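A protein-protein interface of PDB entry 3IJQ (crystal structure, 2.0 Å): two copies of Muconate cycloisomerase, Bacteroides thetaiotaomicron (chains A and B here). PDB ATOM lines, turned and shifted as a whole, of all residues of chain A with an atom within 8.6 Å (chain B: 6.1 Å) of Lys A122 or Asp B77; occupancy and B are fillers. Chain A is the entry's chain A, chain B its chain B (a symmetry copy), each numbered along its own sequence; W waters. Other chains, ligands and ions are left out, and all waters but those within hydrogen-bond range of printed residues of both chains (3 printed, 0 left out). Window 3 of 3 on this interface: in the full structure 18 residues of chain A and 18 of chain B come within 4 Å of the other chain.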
ATOM      1  N   TYR A 113      11.466   5.146   8.751  1.00  0.00           N
ATOM      2  CA  TYR A 113      10.822   6.404   8.392  1.00  0.00           C
ATOM      3  C   TYR A 113      10.294   6.293   6.958  1.00  0.00           C
ATOM      4  O   TYR A 113       9.264   6.880   6.606  1.00  0.00           O
ATOM      5  CB  TYR A 113      11.806   7.584   8.503  1.00  0.00           C
ATOM      6  CG  TYR A 113      12.819   7.706   7.377  1.00  0.00           C
ATOM      7  CD1 TYR A 113      12.439   8.188   6.121  1.00  0.00           C
ATOM      8  CD2 TYR A 113      14.155   7.338   7.563  1.00  0.00           C
ATOM      9  CE1 TYR A 113      13.353   8.294   5.083  1.00  0.00           C
ATOM     10  CE2 TYR A 113      15.086   7.445   6.524  1.00  0.00           C
ATOM     11  CZ  TYR A 113      14.669   7.918   5.288  1.00  0.00           C
ATOM     12  OH  TYR A 113      15.546   7.968   4.234  1.00  0.00           O
ATOM     13  N   TRP A 116       7.351   3.843   6.757  1.00  0.00           N
ATOM     14  CA  TRP A 116       6.189   4.572   7.249  1.00  0.00           C
ATOM     15  C   TRP A 116       5.786   5.707   6.305  1.00  0.00           C
ATOM     16  O   TRP A 116       4.829   6.420   6.576  1.00  0.00           O
ATOM     17  CB  TRP A 116       6.457   5.148   8.642  1.00  0.00           C
ATOM     18  CG  TRP A 116       6.435   4.140   9.783  1.00  0.00           C
ATOM     19  CD1 TRP A 116       5.619   3.042   9.913  1.00  0.00           C
ATOM     20  CD2 TRP A 116       7.203   4.212  10.995  1.00  0.00           C
ATOM     21  NE1 TRP A 116       5.832   2.436  11.131  1.00  0.00           N
ATOM     22  CE2 TRP A 116       6.797   3.132  11.814  1.00  0.00           C
ATOM     23  CE3 TRP A 116       8.194   5.089  11.467  1.00  0.00           C
ATOM     24  CZ2 TRP A 116       7.349   2.903  13.086  1.00  0.00           C
ATOM     25  CZ3 TRP A 116       8.745   4.861  12.740  1.00  0.00           C
ATOM     26  CH2 TRP A 116       8.319   3.779  13.528  1.00  0.00           C
ATOM     27  N   GLY A 117       6.531   5.876   5.213  1.00  0.00           N
ATOM     28  CA  GLY A 117       6.224   6.908   4.229  1.00  0.00           C
ATOM     29  C   GLY A 117       6.487   8.363   4.594  1.00  0.00           C
ATOM     30  O   GLY A 117       5.865   9.269   4.031  1.00  0.00           O
ATOM     31  N   LEU A 118       7.421   8.606   5.510  1.00  0.00           N
ATOM     32  CA  LEU A 118       7.723   9.972   5.948  1.00  0.00           C
ATOM     33  C   LEU A 118       8.863  10.620   5.163  1.00  0.00           C
ATOM     34  O   LEU A 118       9.643   9.934   4.511  1.00  0.00           O
ATOM     35  CB  LEU A 118       8.074   9.961   7.439  1.00  0.00           C
ATOM     36  CG  LEU A 118       7.048   9.288   8.356  1.00  0.00           C
ATOM     37  CD1 LEU A 118       7.612   9.138   9.762  1.00  0.00           C
ATOM     38  CD2 LEU A 118       5.770  10.112   8.370  1.00  0.00           C
ATOM     39  N   ASN A 119       8.949  11.944   5.235  1.00  0.00           N
ATOM     40  CA  ASN A 119       9.994  12.716   4.548  1.00  0.00           C
ATOM     41  C   ASN A 119      11.120  13.016   5.557  1.00  0.00           C
ATOM     42  O   ASN A 119      10.944  13.850   6.437  1.00  0.00           O
ATOM     43  CB  ASN A 119       9.390  14.027   4.035  1.00  0.00           C
ATOM     44  CG  ASN A 119      10.378  14.869   3.244  1.00  0.00           C
ATOM     45  OD1 ASN A 119      11.592  14.773   3.434  1.00  0.00           O
ATOM     46  ND2 ASN A 119       9.855  15.723   2.366  1.00  0.00           N
ATOM     47  N   LYS A 120      12.262  12.346   5.431  1.00  0.00           N
ATOM     48  CA  LYS A 120      13.376  12.538   6.371  1.00  0.00           C
ATOM     49  C   LYS A 120      13.858  13.983   6.470  1.00  0.00           C
ATOM     50  O   LYS A 120      14.515  14.361   7.439  1.00  0.00           O
ATOM     51  CB  LYS A 120      14.564  11.642   5.999  1.00  0.00           C
ATOM     52  CG  LYS A 120      15.230  12.031   4.688  1.00  0.00           C
ATOM     53  CD  LYS A 120      16.377  11.100   4.316  1.00  0.00           C
ATOM     54  CE  LYS A 120      17.509  11.189   5.312  1.00  0.00           C
ATOM     55  NZ  LYS A 120      18.739  10.512   4.826  1.00  0.00           N
ATOM     56  N   GLU A 121      13.534  14.792   5.469  1.00  0.00           N
ATOM     57  CA  GLU A 121      13.947  16.189   5.489  1.00  0.00           C
ATOM     58  C   GLU A 121      13.089  16.979   6.458  1.00  0.00           C
ATOM     59  O   GLU A 121      13.387  18.130   6.760  1.00  0.00           O
ATOM     60  CB  GLU A 121      13.829  16.816   4.096  1.00  0.00           C
ATOM     61  CG  GLU A 121      14.676  16.149   3.032  1.00  0.00           C
ATOM     62  CD  GLU A 121      16.129  16.034   3.435  1.00  0.00           C
ATOM     63  OE1 GLU A 121      16.689  17.043   3.911  1.00  0.00           O
ATOM     64  OE2 GLU A 121      16.716  14.939   3.274  1.00  0.00           O
ATOM     65  N   LYS A 122      12.021  16.368   6.949  1.00  0.00           N
ATOM     66  CA  LYS A 122      11.146  17.063   7.865  1.00  0.00           C
ATOM     67  C   LYS A 122      11.390  16.724   9.314  1.00  0.00           C
ATOM     68  O   LYS A 122      10.536  16.975  10.162  1.00  0.00           O
ATOM     69  CB  LYS A 122       9.686  16.805   7.506  1.00  0.00           C
ATOM     70  CG  LYS A 122       9.296  17.425   6.180  1.00  0.00           C
ATOM     71  CD  LYS A 122       7.816  17.266   5.921  1.00  0.00           C
ATOM     72  CE  LYS A 122       7.433  17.922   4.615  1.00  0.00           C
ATOM     73  NZ  LYS A 122       6.006  17.654   4.319  1.00  0.00           N
ATOM     74  N   THR A 123      12.556  16.151   9.598  1.00  0.00           N
ATOM     75  CA  THR A 123      12.922  15.825  10.966  1.00  0.00           C
ATOM     76  C   THR A 123      12.987  17.157  11.706  1.00  0.00           C
ATOM     77  O   THR A 123      13.308  18.191  11.119  1.00  0.00           O
ATOM     78  CB  THR A 123      14.299  15.154  11.028  1.00  0.00           C
ATOM     79  OG1 THR A 123      15.241  15.929  10.274  1.00  0.00           O
ATOM     80  CG2 THR A 123      14.236  13.745  10.462  1.00  0.00           C
ATOM     81  N   PRO A 124      12.688  17.149  13.010  1.00  0.00           N
ATOM     82  CA  PRO A 124      12.712  18.371  13.814  1.00  0.00           C
ATOM     83  C   PRO A 124      14.073  18.700  14.425  1.00  0.00           C
ATOM     84  O   PRO A 124      15.031  17.927  14.318  1.00  0.00           O
ATOM     85  CB  PRO A 124      11.684  18.071  14.888  1.00  0.00           C
ATOM     86  CG  PRO A 124      12.019  16.618  15.204  1.00  0.00           C
ATOM     87  CD  PRO A 124      12.201  16.005  13.806  1.00  0.00           C
ATOM     88  N   SER A 125      14.149  19.872  15.050  1.00  0.00           N
ATOM     89  CA  SER A 125      15.356  20.289  15.739  1.00  0.00           C
ATOM     90  C   SER A 125      15.192  19.610  17.088  1.00  0.00           C
ATOM     91  O   SER A 125      14.071  19.485  17.567  1.00  0.00           O
ATOM     92  CB  SER A 125      15.372  21.806  15.966  1.00  0.00           C
ATOM     93  OG  SER A 125      15.373  22.537  14.754  1.00  0.00           O
ATOM     94  N   SER A 293      13.831   8.279  16.371  1.00  0.00           N
ATOM     95  CA  SER A 293      14.019   9.332  15.375  1.00  0.00           C
ATOM     96  C   SER A 293      13.350   8.977  14.055  1.00  0.00           C
ATOM     97  O   SER A 293      13.040   9.861  13.255  1.00  0.00           O
ATOM     98  CB  SER A 293      15.510   9.576  15.133  1.00  0.00           C
ATOM     99  OG  SER A 293      16.156  10.024  16.312  1.00  0.00           O
ATOM    100  N   PHE A 295      10.420   8.194  13.401  1.00  0.00           N
ATOM    101  CA  PHE A 295       9.109   8.793  13.195  1.00  0.00           C
ATOM    102  C   PHE A 295       9.090  10.268  13.603  1.00  0.00           C
ATOM    103  O   PHE A 295       8.028  10.888  13.663  1.00  0.00           O
ATOM    104  CB  PHE A 295       8.007   8.008  13.933  1.00  0.00           C
ATOM    105  CG  PHE A 295       8.144   8.000  15.428  1.00  0.00           C
ATOM    106  CD1 PHE A 295       7.658   9.054  16.193  1.00  0.00           C
ATOM    107  CD2 PHE A 295       8.728   6.919  16.075  1.00  0.00           C
ATOM    108  CE1 PHE A 295       7.751   9.029  17.592  1.00  0.00           C
ATOM    109  CE2 PHE A 295       8.826   6.885  17.474  1.00  0.00           C
ATOM    110  CZ  PHE A 295       8.337   7.940  18.226  1.00  0.00           C
ATOM    111  N   SER A 296      10.268  10.833  13.860  1.00  0.00           N
ATOM    112  CA  SER A 296      10.355  12.236  14.252  1.00  0.00           C
ATOM    113  C   SER A 296       9.829  13.203  13.184  1.00  0.00           C
ATOM    114  O   SER A 296       9.430  14.325  13.503  1.00  0.00           O
ATOM    115  CB  SER A 296      11.794  12.616  14.626  1.00  0.00           C
ATOM    116  OG  SER A 296      12.673  12.496  13.524  1.00  0.00           O
ATOM    117  N   PRO A 297       9.826  12.798  11.902  1.00  0.00           N
ATOM    118  CA  PRO A 297       9.312  13.736  10.897  1.00  0.00           C
ATOM    119  C   PRO A 297       7.829  14.040  11.108  1.00  0.00           C
ATOM    120  O   PRO A 297       7.295  14.986  10.534  1.00  0.00           O
ATOM    121  CB  PRO A 297       9.544  12.997   9.582  1.00  0.00           C
ATOM    122  CG  PRO A 297      10.774  12.212   9.867  1.00  0.00           C
ATOM    123  CD  PRO A 297      10.499  11.662  11.246  1.00  0.00           C
ATOM    124  N   ALA A 298       7.174  13.237  11.942  1.00  0.00           N
ATOM    125  CA  ALA A 298       5.749  13.406  12.207  1.00  0.00           C
ATOM    126  C   ALA A 298       5.439  14.074  13.553  1.00  0.00           C
ATOM    127  O   ALA A 298       4.277  14.221  13.910  1.00  0.00           O
ATOM    128  CB  ALA A 298       5.048  12.045  12.124  1.00  0.00           C
ATOM    129  N   VAL A 299       6.467  14.479  14.293  1.00  0.00           N
ATOM    130  CA  VAL A 299       6.258  15.119  15.591  1.00  0.00           C
ATOM    131  C   VAL A 299       6.520  16.624  15.533  1.00  0.00           C
ATOM    132  O   VAL A 299       7.156  17.123  14.600  1.00  0.00           O
ATOM    133  CB  VAL A 299       7.170  14.499  16.677  1.00  0.00           C
ATOM    134  CG1 VAL A 299       7.038  12.981  16.665  1.00  0.00           C
ATOM    135  CG2 VAL A 299       8.613  14.923  16.456  1.00  0.00           C
ATOM    136  N   ASP A 300       6.033  17.345  16.538  1.00  0.00           N
ATOM    137  CA  ASP A 300       6.204  18.790  16.587  1.00  0.00           C
ATOM    138  C   ASP A 300       7.457  19.216  17.359  1.00  0.00           C
ATOM    139  O   ASP A 300       8.150  20.153  16.965  1.00  0.00           O
ATOM    140  CB  ASP A 300       4.954  19.433  17.192  1.00  0.00           C
ATOM    141  CG  ASP A 300       3.714  19.255  16.316  1.00  0.00           C
ATOM    142  OD1 ASP A 300       3.199  18.117  16.178  1.00  0.00           O
ATOM    143  OD2 ASP A 300       3.253  20.270  15.760  1.00  0.00           O
ATOM    144  N   LYS A 324      19.445  19.921  13.738  1.00  0.00           N
ATOM    145  CA  LYS A 324      18.399  18.982  13.320  1.00  0.00           C
ATOM    146  C   LYS A 324      18.704  17.515  13.538  1.00  0.00           C
ATOM    147  O   LYS A 324      19.848  17.083  13.401  1.00  0.00           O
ATOM    148  CB  LYS A 324      18.073  19.157  11.832  1.00  0.00           C
ATOM    149  CG  LYS A 324      17.201  20.344  11.472  1.00  0.00           C
ATOM    150  CD  LYS A 324      16.687  20.192  10.033  1.00  0.00           C
ATOM    151  CE  LYS A 324      15.970  18.850   9.860  1.00  0.00           C
ATOM    152  NZ  LYS A 324      15.362  18.628   8.521  1.00  0.00           N
ATOM    153  N   ILE A 325      17.677  16.741  13.879  1.00  0.00           N
ATOM    154  CA  ILE A 325      17.864  15.308  14.032  1.00  0.00           C
ATOM    155  C   ILE A 325      18.058  14.892  12.587  1.00  0.00           C
ATOM    156  O   ILE A 325      17.267  15.268  11.718  1.00  0.00           O
ATOM    157  CB  ILE A 325      16.623  14.634  14.616  1.00  0.00           C
ATOM    158  CG1 ILE A 325      16.644  14.774  16.141  1.00  0.00           C
ATOM    159  CG2 ILE A 325      16.581  13.166  14.205  1.00  0.00           C
ATOM    160  CD1 ILE A 325      17.850  14.111  16.801  1.00  0.00           C
ATOM    161  N   LEU A 327      18.515  11.760   9.946  1.00  0.00           N
ATOM    162  CA  LEU A 327      18.421  10.342   9.628  1.00  0.00           C
ATOM    163  C   LEU A 327      19.338   9.946   8.479  1.00  0.00           C
ATOM    164  O   LEU A 327      19.474  10.682   7.497  1.00  0.00           O
ATOM    165  CB  LEU A 327      16.985   9.990   9.240  1.00  0.00           C
ATOM    166  CG  LEU A 327      15.946  10.084  10.349  1.00  0.00           C
ATOM    167  CD1 LEU A 327      14.563  10.247   9.740  1.00  0.00           C
ATOM    168  CD2 LEU A 327      16.042   8.828  11.228  1.00  0.00           C
ATOM    169  N   PHE B  69       7.060  14.715  -8.058  1.00  0.00           N
ATOM    170  CA  PHE B  69       7.568  13.860  -6.992  1.00  0.00           C
ATOM    171  C   PHE B  69       8.547  12.837  -7.552  1.00  0.00           C
ATOM    172  O   PHE B  69       8.214  12.078  -8.457  1.00  0.00           O
ATOM    173  CB  PHE B  69       6.408  13.164  -6.293  1.00  0.00           C
ATOM    174  CG  PHE B  69       5.503  14.108  -5.570  1.00  0.00           C
ATOM    175  CD1 PHE B  69       5.940  14.766  -4.427  1.00  0.00           C
ATOM    176  CD2 PHE B  69       4.225  14.370  -6.051  1.00  0.00           C
ATOM    177  CE1 PHE B  69       5.124  15.675  -3.774  1.00  0.00           C
ATOM    178  CE2 PHE B  69       3.396  15.279  -5.404  1.00  0.00           C
ATOM    179  CZ  PHE B  69       3.845  15.934  -4.266  1.00  0.00           C
ATOM    180  N   GLN B  74       7.416   8.709  -0.382  1.00  0.00           N
ATOM    181  CA  GLN B  74       6.894   9.812   0.415  1.00  0.00           C
ATOM    182  C   GLN B  74       5.366   9.833   0.326  1.00  0.00           C
ATOM    183  O   GLN B  74       4.756  10.781  -0.190  1.00  0.00           O
ATOM    184  CB  GLN B  74       7.481  11.141  -0.069  1.00  0.00           C
ATOM    185  CG  GLN B  74       8.545  11.698   0.868  1.00  0.00           C
ATOM    186  CD  GLN B  74       9.856  11.972   0.174  1.00  0.00           C
ATOM    187  OE1 GLN B  74       9.919  12.755  -0.780  1.00  0.00           O
ATOM    188  NE2 GLN B  74      10.919  11.334   0.651  1.00  0.00           N
ATOM    189  N   LEU B  75       4.749   8.777   0.841  1.00  0.00           N
ATOM    190  CA  LEU B  75       3.302   8.665   0.798  1.00  0.00           C
ATOM    191  C   LEU B  75       2.620   9.698   1.680  1.00  0.00           C
ATOM    192  O   LEU B  75       1.506  10.123   1.385  1.00  0.00           O
ATOM    193  CB  LEU B  75       2.871   7.242   1.184  1.00  0.00           C
ATOM    194  CG  LEU B  75       3.436   6.140   0.276  1.00  0.00           C
ATOM    195  CD1 LEU B  75       2.885   4.783   0.697  1.00  0.00           C
ATOM    196  CD2 LEU B  75       3.072   6.435  -1.188  1.00  0.00           C
ATOM    197  N   GLU B  76       3.279  10.116   2.760  1.00  0.00           N
ATOM    198  CA  GLU B  76       2.678  11.122   3.638  1.00  0.00           C
ATOM    199  C   GLU B  76       2.558  12.457   2.887  1.00  0.00           C
ATOM    200  O   GLU B  76       1.473  13.036   2.801  1.00  0.00           O
ATOM    201  CB  GLU B  76       3.525  11.315   4.895  1.00  0.00           C
ATOM    202  CG  GLU B  76       2.953  12.307   5.907  1.00  0.00           C
ATOM    203  CD  GLU B  76       1.589  11.893   6.435  1.00  0.00           C
ATOM    204  OE1 GLU B  76       1.409  10.697   6.727  1.00  0.00           O
ATOM    205  OE2 GLU B  76       0.697  12.762   6.566  1.00  0.00           O
ATOM    206  N   ASP B  77       3.673  12.934   2.337  1.00  0.00           N
ATOM    207  CA  ASP B  77       3.683  14.197   1.600  1.00  0.00           C
ATOM    208  C   ASP B  77       2.841  14.135   0.328  1.00  0.00           C
ATOM    209  O   ASP B  77       2.080  15.056   0.037  1.00  0.00           O
ATOM    210  CB  ASP B  77       5.111  14.591   1.200  1.00  0.00           C
ATOM    211  CG  ASP B  77       5.907  15.197   2.344  1.00  0.00           C
ATOM    212  OD1 ASP B  77       5.423  15.213   3.501  1.00  0.00           O
ATOM    213  OD2 ASP B  77       7.033  15.655   2.068  1.00  0.00           O
ATOM    214  N   ILE B  78       2.985  13.053  -0.428  1.00  0.00           N
ATOM    215  CA  ILE B  78       2.262  12.907  -1.686  1.00  0.00           C
ATOM    216  C   ILE B  78       0.748  12.824  -1.553  1.00  0.00           C
ATOM    217  O   ILE B  78       0.022  13.516  -2.269  1.00  0.00           O
ATOM    218  CB  ILE B  78       2.754  11.677  -2.470  1.00  0.00           C
ATOM    219  CG1 ILE B  78       4.202  11.895  -2.910  1.00  0.00           C
ATOM    220  CG2 ILE B  78       1.845  11.432  -3.681  1.00  0.00           C
ATOM    221  CD1 ILE B  78       4.836  10.690  -3.583  1.00  0.00           C
ATOM    222  N   LEU B  79       0.268  11.979  -0.645  1.00  0.00           N
ATOM    223  CA  LEU B  79      -1.170  11.838  -0.454  1.00  0.00           C
ATOM    224  C   LEU B  79      -1.765  13.039   0.277  1.00  0.00           C
ATOM    225  O   LEU B  79      -2.961  13.303   0.174  1.00  0.00           O
ATOM    226  CB  LEU B  79      -1.485  10.528   0.277  1.00  0.00           C
ATOM    227  CG  LEU B  79      -1.083   9.300  -0.556  1.00  0.00           C
ATOM    228  CD1 LEU B  79      -1.231   8.020   0.255  1.00  0.00           C
ATOM    229  CD2 LEU B  79      -1.947   9.248  -1.807  1.00  0.00           C
ATOM    230  N   SER B  80      -0.940  13.773   1.009  1.00  0.00           N
ATOM    231  CA  SER B  80      -1.429  14.965   1.696  1.00  0.00           C
ATOM    232  C   SER B  80      -1.661  16.040   0.619  1.00  0.00           C
ATOM    233  O   SER B  80      -2.617  16.820   0.677  1.00  0.00           O
ATOM    234  CB  SER B  80      -0.405  15.453   2.714  1.00  0.00           C
ATOM    235  OG  SER B  80      -0.834  16.671   3.292  1.00  0.00           O
ATOM    236  N   TYR B  81      -0.780  16.064  -0.370  1.00  0.00           N
ATOM    237  CA  TYR B  81      -0.899  17.000  -1.478  1.00  0.00           C
ATOM    238  C   TYR B  81      -2.156  16.629  -2.288  1.00  0.00           C
ATOM    239  O   TYR B  81      -2.967  17.493  -2.633  1.00  0.00           O
ATOM    240  CB  TYR B  81       0.365  16.917  -2.357  1.00  0.00           C
ATOM    241  CG  TYR B  81       0.154  17.295  -3.811  1.00  0.00           C
ATOM    242  CD1 TYR B  81      -0.166  18.607  -4.181  1.00  0.00           C
ATOM    243  CD2 TYR B  81       0.227  16.327  -4.812  1.00  0.00           C
ATOM    244  CE1 TYR B  81      -0.418  18.941  -5.516  1.00  0.00           C
ATOM    245  CE2 TYR B  81      -0.017  16.646  -6.137  1.00  0.00           C
ATOM    246  CZ  TYR B  81      -0.343  17.950  -6.484  1.00  0.00           C
ATOM    247  OH  TYR B  81      -0.615  18.240  -7.798  1.00  0.00           O
ATOM    248  N   VAL B  82      -2.315  15.340  -2.578  1.00  0.00           N
ATOM    249  CA  VAL B  82      -3.469  14.867  -3.341  1.00  0.00           C
ATOM    250  C   VAL B  82      -4.771  15.280  -2.651  1.00  0.00           C
ATOM    251  O   VAL B  82      -5.684  15.820  -3.286  1.00  0.00           O
ATOM    252  CB  VAL B  82      -3.431  13.311  -3.516  1.00  0.00           C
ATOM    253  CG1 VAL B  82      -4.788  12.781  -3.996  1.00  0.00           C
ATOM    254  CG2 VAL B  82      -2.352  12.926  -4.525  1.00  0.00           C
HETATM  255  O   HOH W   1       6.538  13.332   5.604  1.00  0.00           O
HETATM  256  O   HOH W   2       6.378  11.768   2.691  1.00  0.00           O
HETATM  257  O   HOH W   3      12.522  11.142   2.838  1.00  0.00           O
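Of the printed residues of chain B, Gly A117 touches Gln B74 (3.8 Å), Leu B75 (3.4 Å) and Glu B76 (3.0 Å). Of the printed residues of chain B, Asn A119 touches Asp B77 (2.8 Å). Of the printed residues of chain B, Lys A122 touches Asp B77 (2.6 Å). Of the printed residues of chain A, Gln B74 touches Gly A117 (3.8 Å). Of the printed residues of chain A, Leu B75 touches Gly A117. Of the printed residues of chain A, Glu B76 touches Gly A117. Of chain A, only Asn A119 and Lys A122 come within 4 Å of Asp B77. Leu B79 touches none of the printed residues of chain A. The nearest residue of chain A that does not touch Asp B77 is Gly A117 (4.6 Å). The nearest printed residue of chain B that does not touch Gly A117 is Asp B77 (4.6 Å).
Water W3 lies within hydrogen-bond range of the side-chain amide nitrogen (NE2) of Gln B74 (2.7 Å) and the backbone NH (N) of Lys A120 (2.9 Å). Water W1 bridges N of Asn A119 (2.8 Å) and OD1 of Asp B77 (3.0 Å). Water W2 lies within hydrogen-bond range of O of Gly A117 (2.9 Å), N of Asp B77 (3.0 Å) and O of Gln B74 (3.5 Å).
No position is printed for both chains.
Among the printed residues, pairs that only touch across the chains: Gly A117 with Gln B74.
Printed residues of chain B that touch a printed residue of chain A: Gln B74, Leu B75, Glu B76 and Asp B77. Of the 21 printed residues of chain A, 3 touch a printed residue of chain B. Printed residues of chain A that touch a printed residue of chain B: Gly A117, Asn A119 and Lys A122. Among the printed residues, Asp or Glu carboxylates within 4 Å of a Lys or Arg side-chain nitrogen of the other chain: Lys A122 with Asp B77.
The side-chain amide oxygen (OD1) of Asn A119 sits at hydrogen-bond distance from the backbone NH (N) of Glu A121 (2.8 Å).
O of Gly A117 lies within hydrogen-bond range of N of Leu B75 (3.4 Å). The backbone NH of Glu B76 lies within hydrogen-bond range of the backbone carbonyl oxygen of Gly A117 (3.0 Å). OD2 of Asp B77 is in hydrogen-bond range of ND2 of Asn A119, at 2.8 Å. NZ of Lys A122 is in salt-bridge range of OD1 of Asp B77, 2.6 Å away.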
